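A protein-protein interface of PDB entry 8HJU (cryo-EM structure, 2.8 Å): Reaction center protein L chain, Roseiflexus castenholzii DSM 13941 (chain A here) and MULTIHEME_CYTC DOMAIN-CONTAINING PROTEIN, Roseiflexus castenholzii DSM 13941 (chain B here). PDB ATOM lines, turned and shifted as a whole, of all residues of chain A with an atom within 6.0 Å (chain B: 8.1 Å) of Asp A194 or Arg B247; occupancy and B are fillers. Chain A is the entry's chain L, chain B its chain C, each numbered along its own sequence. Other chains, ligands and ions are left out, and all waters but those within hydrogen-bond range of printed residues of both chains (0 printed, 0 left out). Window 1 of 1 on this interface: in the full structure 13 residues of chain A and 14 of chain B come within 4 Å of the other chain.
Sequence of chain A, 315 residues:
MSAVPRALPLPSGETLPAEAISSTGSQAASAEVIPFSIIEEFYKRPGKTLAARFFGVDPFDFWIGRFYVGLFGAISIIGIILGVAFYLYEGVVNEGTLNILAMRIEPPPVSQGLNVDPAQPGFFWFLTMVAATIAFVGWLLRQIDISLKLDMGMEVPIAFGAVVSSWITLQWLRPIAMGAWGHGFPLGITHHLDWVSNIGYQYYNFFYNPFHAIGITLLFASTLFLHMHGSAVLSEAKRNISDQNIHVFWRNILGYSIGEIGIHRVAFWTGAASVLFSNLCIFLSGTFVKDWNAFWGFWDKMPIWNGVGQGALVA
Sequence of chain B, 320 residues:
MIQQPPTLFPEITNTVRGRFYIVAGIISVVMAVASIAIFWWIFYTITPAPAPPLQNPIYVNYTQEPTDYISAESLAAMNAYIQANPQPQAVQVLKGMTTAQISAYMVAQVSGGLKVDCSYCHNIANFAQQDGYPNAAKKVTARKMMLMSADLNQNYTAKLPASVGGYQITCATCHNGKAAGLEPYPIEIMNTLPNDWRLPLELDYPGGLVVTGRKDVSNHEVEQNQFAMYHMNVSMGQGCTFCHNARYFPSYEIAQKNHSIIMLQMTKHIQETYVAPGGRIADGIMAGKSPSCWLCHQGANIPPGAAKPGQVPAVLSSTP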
ATOM      1  N   THR A 190      25.662  -7.279  -4.766  1.00  0.00           N
ATOM      2  CA  THR A 190      25.324  -5.874  -4.983  1.00  0.00           C
ATOM      3  C   THR A 190      23.904  -5.542  -4.552  1.00  0.00           C
ATOM      4  O   THR A 190      23.553  -4.363  -4.484  1.00  0.00           O
ATOM      5  CB  THR A 190      25.501  -5.441  -6.444  1.00  0.00           C
ATOM      6  OG1 THR A 190      24.391  -5.915  -7.215  1.00  0.00           O
ATOM      7  CG2 THR A 190      26.799  -5.955  -7.032  1.00  0.00           C
ATOM      8  N   HIS A 191      23.082  -6.536  -4.229  1.00  0.00           N
ATOM      9  CA  HIS A 191      21.734  -6.225  -3.775  1.00  0.00           C
ATOM     10  C   HIS A 191      21.539  -6.421  -2.287  1.00  0.00           C
ATOM     11  O   HIS A 191      20.699  -5.741  -1.694  1.00  0.00           O
ATOM     12  CB  HIS A 191      20.680  -7.050  -4.508  1.00  0.00           C
ATOM     13  CG  HIS A 191      19.281  -6.667  -4.145  1.00  0.00           C
ATOM     14  ND1 HIS A 191      18.720  -5.468  -4.522  1.00  0.00           N
ATOM     15  CD2 HIS A 191      18.346  -7.300  -3.402  1.00  0.00           C
ATOM     16  CE1 HIS A 191      17.492  -5.388  -4.048  1.00  0.00           C
ATOM     17  NE2 HIS A 191      17.240  -6.488  -3.364  1.00  0.00           N
ATOM     18  N   HIS A 192      22.278  -7.331  -1.658  1.00  0.00           N
ATOM     19  CA  HIS A 192      22.287  -7.325  -0.206  1.00  0.00           C
ATOM     20  C   HIS A 192      22.837  -6.006   0.311  1.00  0.00           C
ATOM     21  O   HIS A 192      22.529  -5.604   1.437  1.00  0.00           O
ATOM     22  CB  HIS A 192      23.085  -8.511   0.332  1.00  0.00           C
ATOM     23  CG  HIS A 192      24.525  -8.501  -0.052  1.00  0.00           C
ATOM     24  ND1 HIS A 192      24.945  -8.554  -1.361  1.00  0.00           N
ATOM     25  CD2 HIS A 192      25.646  -8.442   0.699  1.00  0.00           C
ATOM     26  CE1 HIS A 192      26.262  -8.523  -1.400  1.00  0.00           C
ATOM     27  NE2 HIS A 192      26.712  -8.454  -0.164  1.00  0.00           N
ATOM     28  N   LEU A 193      23.620  -5.302  -0.508  1.00  0.00           N
ATOM     29  CA  LEU A 193      24.043  -3.954  -0.156  1.00  0.00           C
ATOM     30  C   LEU A 193      22.870  -2.992  -0.133  1.00  0.00           C
ATOM     31  O   LEU A 193      22.859  -2.057   0.667  1.00  0.00           O
ATOM     32  CB  LEU A 193      25.097  -3.452  -1.134  1.00  0.00           C
ATOM     33  CG  LEU A 193      26.288  -4.354  -1.410  1.00  0.00           C
ATOM     34  CD1 LEU A 193      27.320  -3.587  -2.195  1.00  0.00           C
ATOM     35  CD2 LEU A 193      26.862  -4.852  -0.123  1.00  0.00           C
ATOM     36  N   ASP A 194      21.881  -3.200  -1.000  1.00  0.00           N
ATOM     37  CA  ASP A 194      20.681  -2.373  -0.959  1.00  0.00           C
ATOM     38  C   ASP A 194      19.922  -2.591   0.334  1.00  0.00           C
ATOM     39  O   ASP A 194      19.412  -1.639   0.931  1.00  0.00           O
ATOM     40  CB  ASP A 194      19.795  -2.680  -2.158  1.00  0.00           C
ATOM     41  CG  ASP A 194      20.511  -2.492  -3.462  1.00  0.00           C
ATOM     42  OD1 ASP A 194      21.617  -1.925  -3.448  1.00  0.00           O
ATOM     43  OD2 ASP A 194      19.975  -2.906  -4.503  1.00  0.00           O
ATOM     44  N   TRP A 195      19.858  -3.838   0.795  1.00  0.00           N
ATOM     45  CA  TRP A 195      19.256  -4.116   2.088  1.00  0.00           C
ATOM     46  C   TRP A 195      20.057  -3.489   3.216  1.00  0.00           C
ATOM     47  O   TRP A 195      19.483  -2.937   4.155  1.00  0.00           O
ATOM     48  CB  TRP A 195      19.149  -5.620   2.292  1.00  0.00           C
ATOM     49  CG  TRP A 195      18.528  -6.031   3.582  1.00  0.00           C
ATOM     50  CD1 TRP A 195      17.218  -6.287   3.806  1.00  0.00           C
ATOM     51  CD2 TRP A 195      19.199  -6.255   4.821  1.00  0.00           C
ATOM     52  NE1 TRP A 195      17.021  -6.654   5.110  1.00  0.00           N
ATOM     53  CE2 TRP A 195      18.227  -6.644   5.755  1.00  0.00           C
ATOM     54  CE3 TRP A 195      20.528  -6.162   5.232  1.00  0.00           C
ATOM     55  CZ2 TRP A 195      18.539  -6.938   7.071  1.00  0.00           C
ATOM     56  CZ3 TRP A 195      20.834  -6.456   6.533  1.00  0.00           C
ATOM     57  CH2 TRP A 195      19.847  -6.839   7.440  1.00  0.00           C
ATOM     58  N   VAL A 196      21.384  -3.585   3.157  1.00  0.00           N
ATOM     59  CA  VAL A 196      22.208  -3.017   4.217  1.00  0.00           C
ATOM     60  C   VAL A 196      22.037  -1.508   4.266  1.00  0.00           C
ATOM     61  O   VAL A 196      21.977  -0.913   5.345  1.00  0.00           O
ATOM     62  CB  VAL A 196      23.682  -3.425   4.032  1.00  0.00           C
ATOM     63  CG1 VAL A 196      24.555  -2.720   5.034  1.00  0.00           C
ATOM     64  CG2 VAL A 196      23.840  -4.908   4.203  1.00  0.00           C
ATOM     65  N   SER A 197      21.912  -0.870   3.103  1.00  0.00           N
ATOM     66  CA  SER A 197      21.730   0.576   3.061  1.00  0.00           C
ATOM     67  C   SER A 197      20.345   0.979   3.539  1.00  0.00           C
ATOM     68  O   SER A 197      20.194   1.987   4.234  1.00  0.00           O
ATOM     69  CB  SER A 197      21.965   1.097   1.647  1.00  0.00           C
ATOM     70  OG  SER A 197      22.358   2.454   1.669  1.00  0.00           O
ATOM     71  N   ASN A 198      19.318   0.214   3.171  1.00  0.00           N
ATOM     72  CA  ASN A 198      17.965   0.574   3.566  1.00  0.00           C
ATOM     73  C   ASN A 198      17.707   0.276   5.033  1.00  0.00           C
ATOM     74  O   ASN A 198      16.930   0.984   5.678  1.00  0.00           O
ATOM     75  CB  ASN A 198      16.959  -0.147   2.679  1.00  0.00           C
ATOM     76  CG  ASN A 198      16.840   0.484   1.320  1.00  0.00           C
ATOM     77  OD1 ASN A 198      16.345   1.595   1.188  1.00  0.00           O
ATOM     78  ND2 ASN A 198      17.297  -0.217   0.300  1.00  0.00           N
ATOM     79  N   ILE A 199      18.348  -0.754   5.580  1.00  0.00           N
ATOM     80  CA  ILE A 199      18.256  -1.014   7.008  1.00  0.00           C
ATOM     81  C   ILE A 199      19.076   0.006   7.780  1.00  0.00           C
ATOM     82  O   ILE A 199      18.669   0.473   8.846  1.00  0.00           O
ATOM     83  CB  ILE A 199      18.702  -2.454   7.315  1.00  0.00           C
ATOM     84  CG1 ILE A 199      17.662  -3.448   6.811  1.00  0.00           C
ATOM     85  CG2 ILE A 199      18.912  -2.643   8.792  1.00  0.00           C
ATOM     86  CD1 ILE A 199      16.364  -3.393   7.549  1.00  0.00           C
ATOM     87  N   THR B 241      13.671   5.567   5.329  1.00  0.00           N
ATOM     88  CA  THR B 241      13.135   4.879   4.165  1.00  0.00           C
ATOM     89  C   THR B 241      11.635   5.053   4.016  1.00  0.00           C
ATOM     90  O   THR B 241      11.026   4.356   3.200  1.00  0.00           O
ATOM     91  CB  THR B 241      13.476   3.396   4.237  1.00  0.00           C
ATOM     92  OG1 THR B 241      12.976   2.855   5.461  1.00  0.00           O
ATOM     93  CG2 THR B 241      14.956   3.209   4.199  1.00  0.00           C
ATOM     94  N   HIS B 244      12.265   7.200   0.907  1.00  0.00           N
ATOM     95  CA  HIS B 244      13.491   7.036   0.154  1.00  0.00           C
ATOM     96  C   HIS B 244      13.766   5.560  -0.034  1.00  0.00           C
ATOM     97  O   HIS B 244      13.495   4.756   0.855  1.00  0.00           O
ATOM     98  CB  HIS B 244      14.671   7.682   0.869  1.00  0.00           C
ATOM     99  CG  HIS B 244      14.776   9.159   0.669  1.00  0.00           C
ATOM    100  ND1 HIS B 244      15.013   9.728  -0.559  1.00  0.00           N
ATOM    101  CD2 HIS B 244      14.692  10.182   1.548  1.00  0.00           C
ATOM    102  CE1 HIS B 244      15.065  11.039  -0.429  1.00  0.00           C
ATOM    103  NE2 HIS B 244      14.879  11.342   0.842  1.00  0.00           N
ATOM    104  N   ASN B 245      14.278   5.205  -1.203  1.00  0.00           N
ATOM    105  CA  ASN B 245      15.020   3.965  -1.367  1.00  0.00           C
ATOM    106  C   ASN B 245      16.470   4.332  -1.099  1.00  0.00           C
ATOM    107  O   ASN B 245      17.124   4.961  -1.928  1.00  0.00           O
ATOM    108  CB  ASN B 245      14.821   3.377  -2.756  1.00  0.00           C
ATOM    109  CG  ASN B 245      15.347   1.970  -2.869  1.00  0.00           C
ATOM    110  OD1 ASN B 245      16.306   1.607  -2.208  1.00  0.00           O
ATOM    111  ND2 ASN B 245      14.714   1.168  -3.700  1.00  0.00           N
ATOM    112  N   ALA B 246      16.971   3.961   0.076  1.00  0.00           N
ATOM    113  CA  ALA B 246      18.267   4.448   0.524  1.00  0.00           C
ATOM    114  C   ALA B 246      19.407   4.065  -0.402  1.00  0.00           C
ATOM    115  O   ALA B 246      20.501   4.617  -0.257  1.00  0.00           O
ATOM    116  CB  ALA B 246      18.559   3.938   1.927  1.00  0.00           C
ATOM    117  N   ARG B 247      19.220   3.145  -1.365  1.00  0.00           N
ATOM    118  CA  ARG B 247      20.266   2.868  -2.339  1.00  0.00           C
ATOM    119  C   ARG B 247      20.429   4.016  -3.325  1.00  0.00           C
ATOM    120  O   ARG B 247      21.509   4.192  -3.894  1.00  0.00           O
ATOM    121  CB  ARG B 247      19.983   1.553  -3.063  1.00  0.00           C
ATOM    122  CG  ARG B 247      19.071   1.637  -4.258  1.00  0.00           C
ATOM    123  CD  ARG B 247      18.926   0.274  -4.896  1.00  0.00           C
ATOM    124  NE  ARG B 247      18.139   0.318  -6.119  1.00  0.00           N
ATOM    125  CZ  ARG B 247      18.066  -0.671  -6.999  1.00  0.00           C
ATOM    126  NH1 ARG B 247      18.738  -1.791  -6.799  1.00  0.00           N
ATOM    127  NH2 ARG B 247      17.322  -0.537  -8.081  1.00  0.00           N
ATOM    128  N   TYR B 248      19.388   4.817  -3.523  1.00  0.00           N
ATOM    129  CA  TYR B 248      19.505   6.034  -4.319  1.00  0.00           C
ATOM    130  C   TYR B 248      18.517   7.048  -3.771  1.00  0.00           C
ATOM    131  O   TYR B 248      17.314   6.938  -4.015  1.00  0.00           O
ATOM    132  CB  TYR B 248      19.250   5.766  -5.794  1.00  0.00           C
ATOM    133  CG  TYR B 248      19.791   6.838  -6.701  1.00  0.00           C
ATOM    134  CD1 TYR B 248      21.079   7.315  -6.548  1.00  0.00           C
ATOM    135  CD2 TYR B 248      19.014   7.372  -7.714  1.00  0.00           C
ATOM    136  CE1 TYR B 248      21.579   8.287  -7.378  1.00  0.00           C
ATOM    137  CE2 TYR B 248      19.505   8.344  -8.547  1.00  0.00           C
ATOM    138  CZ  TYR B 248      20.787   8.798  -8.375  1.00  0.00           C
ATOM    139  OH  TYR B 248      21.283   9.771  -9.204  1.00  0.00           O
ATOM    140  N   PHE B 249      19.021   8.029  -3.049  1.00  0.00           N
ATOM    141  CA  PHE B 249      18.181   9.069  -2.474  1.00  0.00           C
ATOM    142  C   PHE B 249      17.563   9.986  -3.527  1.00  0.00           C
ATOM    143  O   PHE B 249      16.427  10.427  -3.341  1.00  0.00           O
ATOM    144  CB  PHE B 249      18.981   9.883  -1.459  1.00  0.00           C
ATOM    145  CG  PHE B 249      19.267   9.141  -0.191  1.00  0.00           C
ATOM    146  CD1 PHE B 249      18.244   8.769   0.651  1.00  0.00           C
ATOM    147  CD2 PHE B 249      20.556   8.812   0.156  1.00  0.00           C
ATOM    148  CE1 PHE B 249      18.500   8.086   1.809  1.00  0.00           C
ATOM    149  CE2 PHE B 249      20.813   8.128   1.315  1.00  0.00           C
ATOM    150  CZ  PHE B 249      19.783   7.764   2.140  1.00  0.00           C
ATOM    151  N   PRO B 250      18.238  10.312  -4.634  1.00  0.00           N
ATOM    152  CA  PRO B 250      17.569  11.116  -5.668  1.00  0.00           C
ATOM    153  C   PRO B 250      16.347  10.461  -6.277  1.00  0.00           C
ATOM    154  O   PRO B 250      15.613  11.137  -7.004  1.00  0.00           O
ATOM    155  CB  PRO B 250      18.662  11.310  -6.719  1.00  0.00           C
ATOM    156  CG  PRO B 250      19.889  11.229  -5.977  1.00  0.00           C
ATOM    157  CD  PRO B 250      19.684  10.240  -4.892  1.00  0.00           C
ATOM    158  N   SER B 251      16.100   9.184  -6.016  1.00  0.00           N
ATOM    159  CA  SER B 251      15.001   8.490  -6.667  1.00  0.00           C
ATOM    160  C   SER B 251      13.680   8.811  -5.988  1.00  0.00           C
ATOM    161  O   SER B 251      13.613   8.976  -4.769  1.00  0.00           O
ATOM    162  CB  SER B 251      15.246   6.986  -6.649  1.00  0.00           C
ATOM    163  OG  SER B 251      14.165   6.294  -7.237  1.00  0.00           O
ATOM    164  N   GLU B 253      11.094   6.752  -5.887  1.00  0.00           N
ATOM    165  CA  GLU B 253      10.471   5.434  -5.874  1.00  0.00           C
ATOM    166  C   GLU B 253       9.244   5.393  -4.973  1.00  0.00           C
ATOM    167  O   GLU B 253       8.197   4.864  -5.357  1.00  0.00           O
ATOM    168  CB  GLU B 253      11.489   4.402  -5.398  1.00  0.00           C
ATOM    169  CG  GLU B 253      12.125   3.569  -6.472  1.00  0.00           C
ATOM    170  CD  GLU B 253      12.702   2.287  -5.912  1.00  0.00           C
ATOM    171  OE1 GLU B 253      12.080   1.712  -4.996  1.00  0.00           O
ATOM    172  OE2 GLU B 253      13.778   1.860  -6.377  1.00  0.00           O
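Of the 10 printed residues of chain A, 3 touch a printed residue of chain B. Hydrophobic or aromatic side chains of chain B within 4 Å of the printed part of chain A: Ala B246.
Among the printed residues, merely in contact across the chains: Asn A198 with Thr B241.
O of Ala B246 is in hydrogen-bond range of OG of Ser A197, at 3.4 Å. The guanidinium group (NH1) of Arg B247 is in salt-bridge range of the side-chain carboxylate (OD2) of Asp A194. The side-chain amide oxygen (OD1) of Asn A198 lies within hydrogen-bond range of the backbone NH (N) of Ala B246 (2.7 Å). The side-chain amide nitrogen (ND2) of Asn A198 is in hydrogen-bond range of the side-chain amide oxygen (OD1) of Asn B245, at 3.3 Å.
The side-chain carboxylate of Asp A194 lies within hydrogen-bond range of a ring nitrogen (ND1) of His A191. The side-chain carboxylate (OE2) of Glu B253 sits at hydrogen-bond distance from the side-chain amide nitrogen (ND2) of Asn B245 (2.9 Å). N of Arg B247 sits close to OD1 of Asn B245, 3.4 Å away. The side-chain amide nitrogen of Asn A198 lies within hydrogen-bond range of the backbone carbonyl oxygen of Asp A194 (2.6 Å).
Of chain B, only Arg B247 comes within 4 Å of Asp A194. Val A196 touches none of the printed residues of chain B. Of the printed residues of chain B, Ser A197 touches Ala B246. Printed residues of chain B within 4 Å of Asn A198: Thr B241, Asn B245 and Ala B246. Printed residues of chain A within 4 Å of Thr B241: Asn A198. Printed residues of chain A within 4 Å of Asn B245: Asn A198. Printed residues of chain A within 4 Å of Ala B246: Ser A197 (3.4 Å) and Asn A198 (2.7 Å). Glu B253 touches none of the printed residues of chain A.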
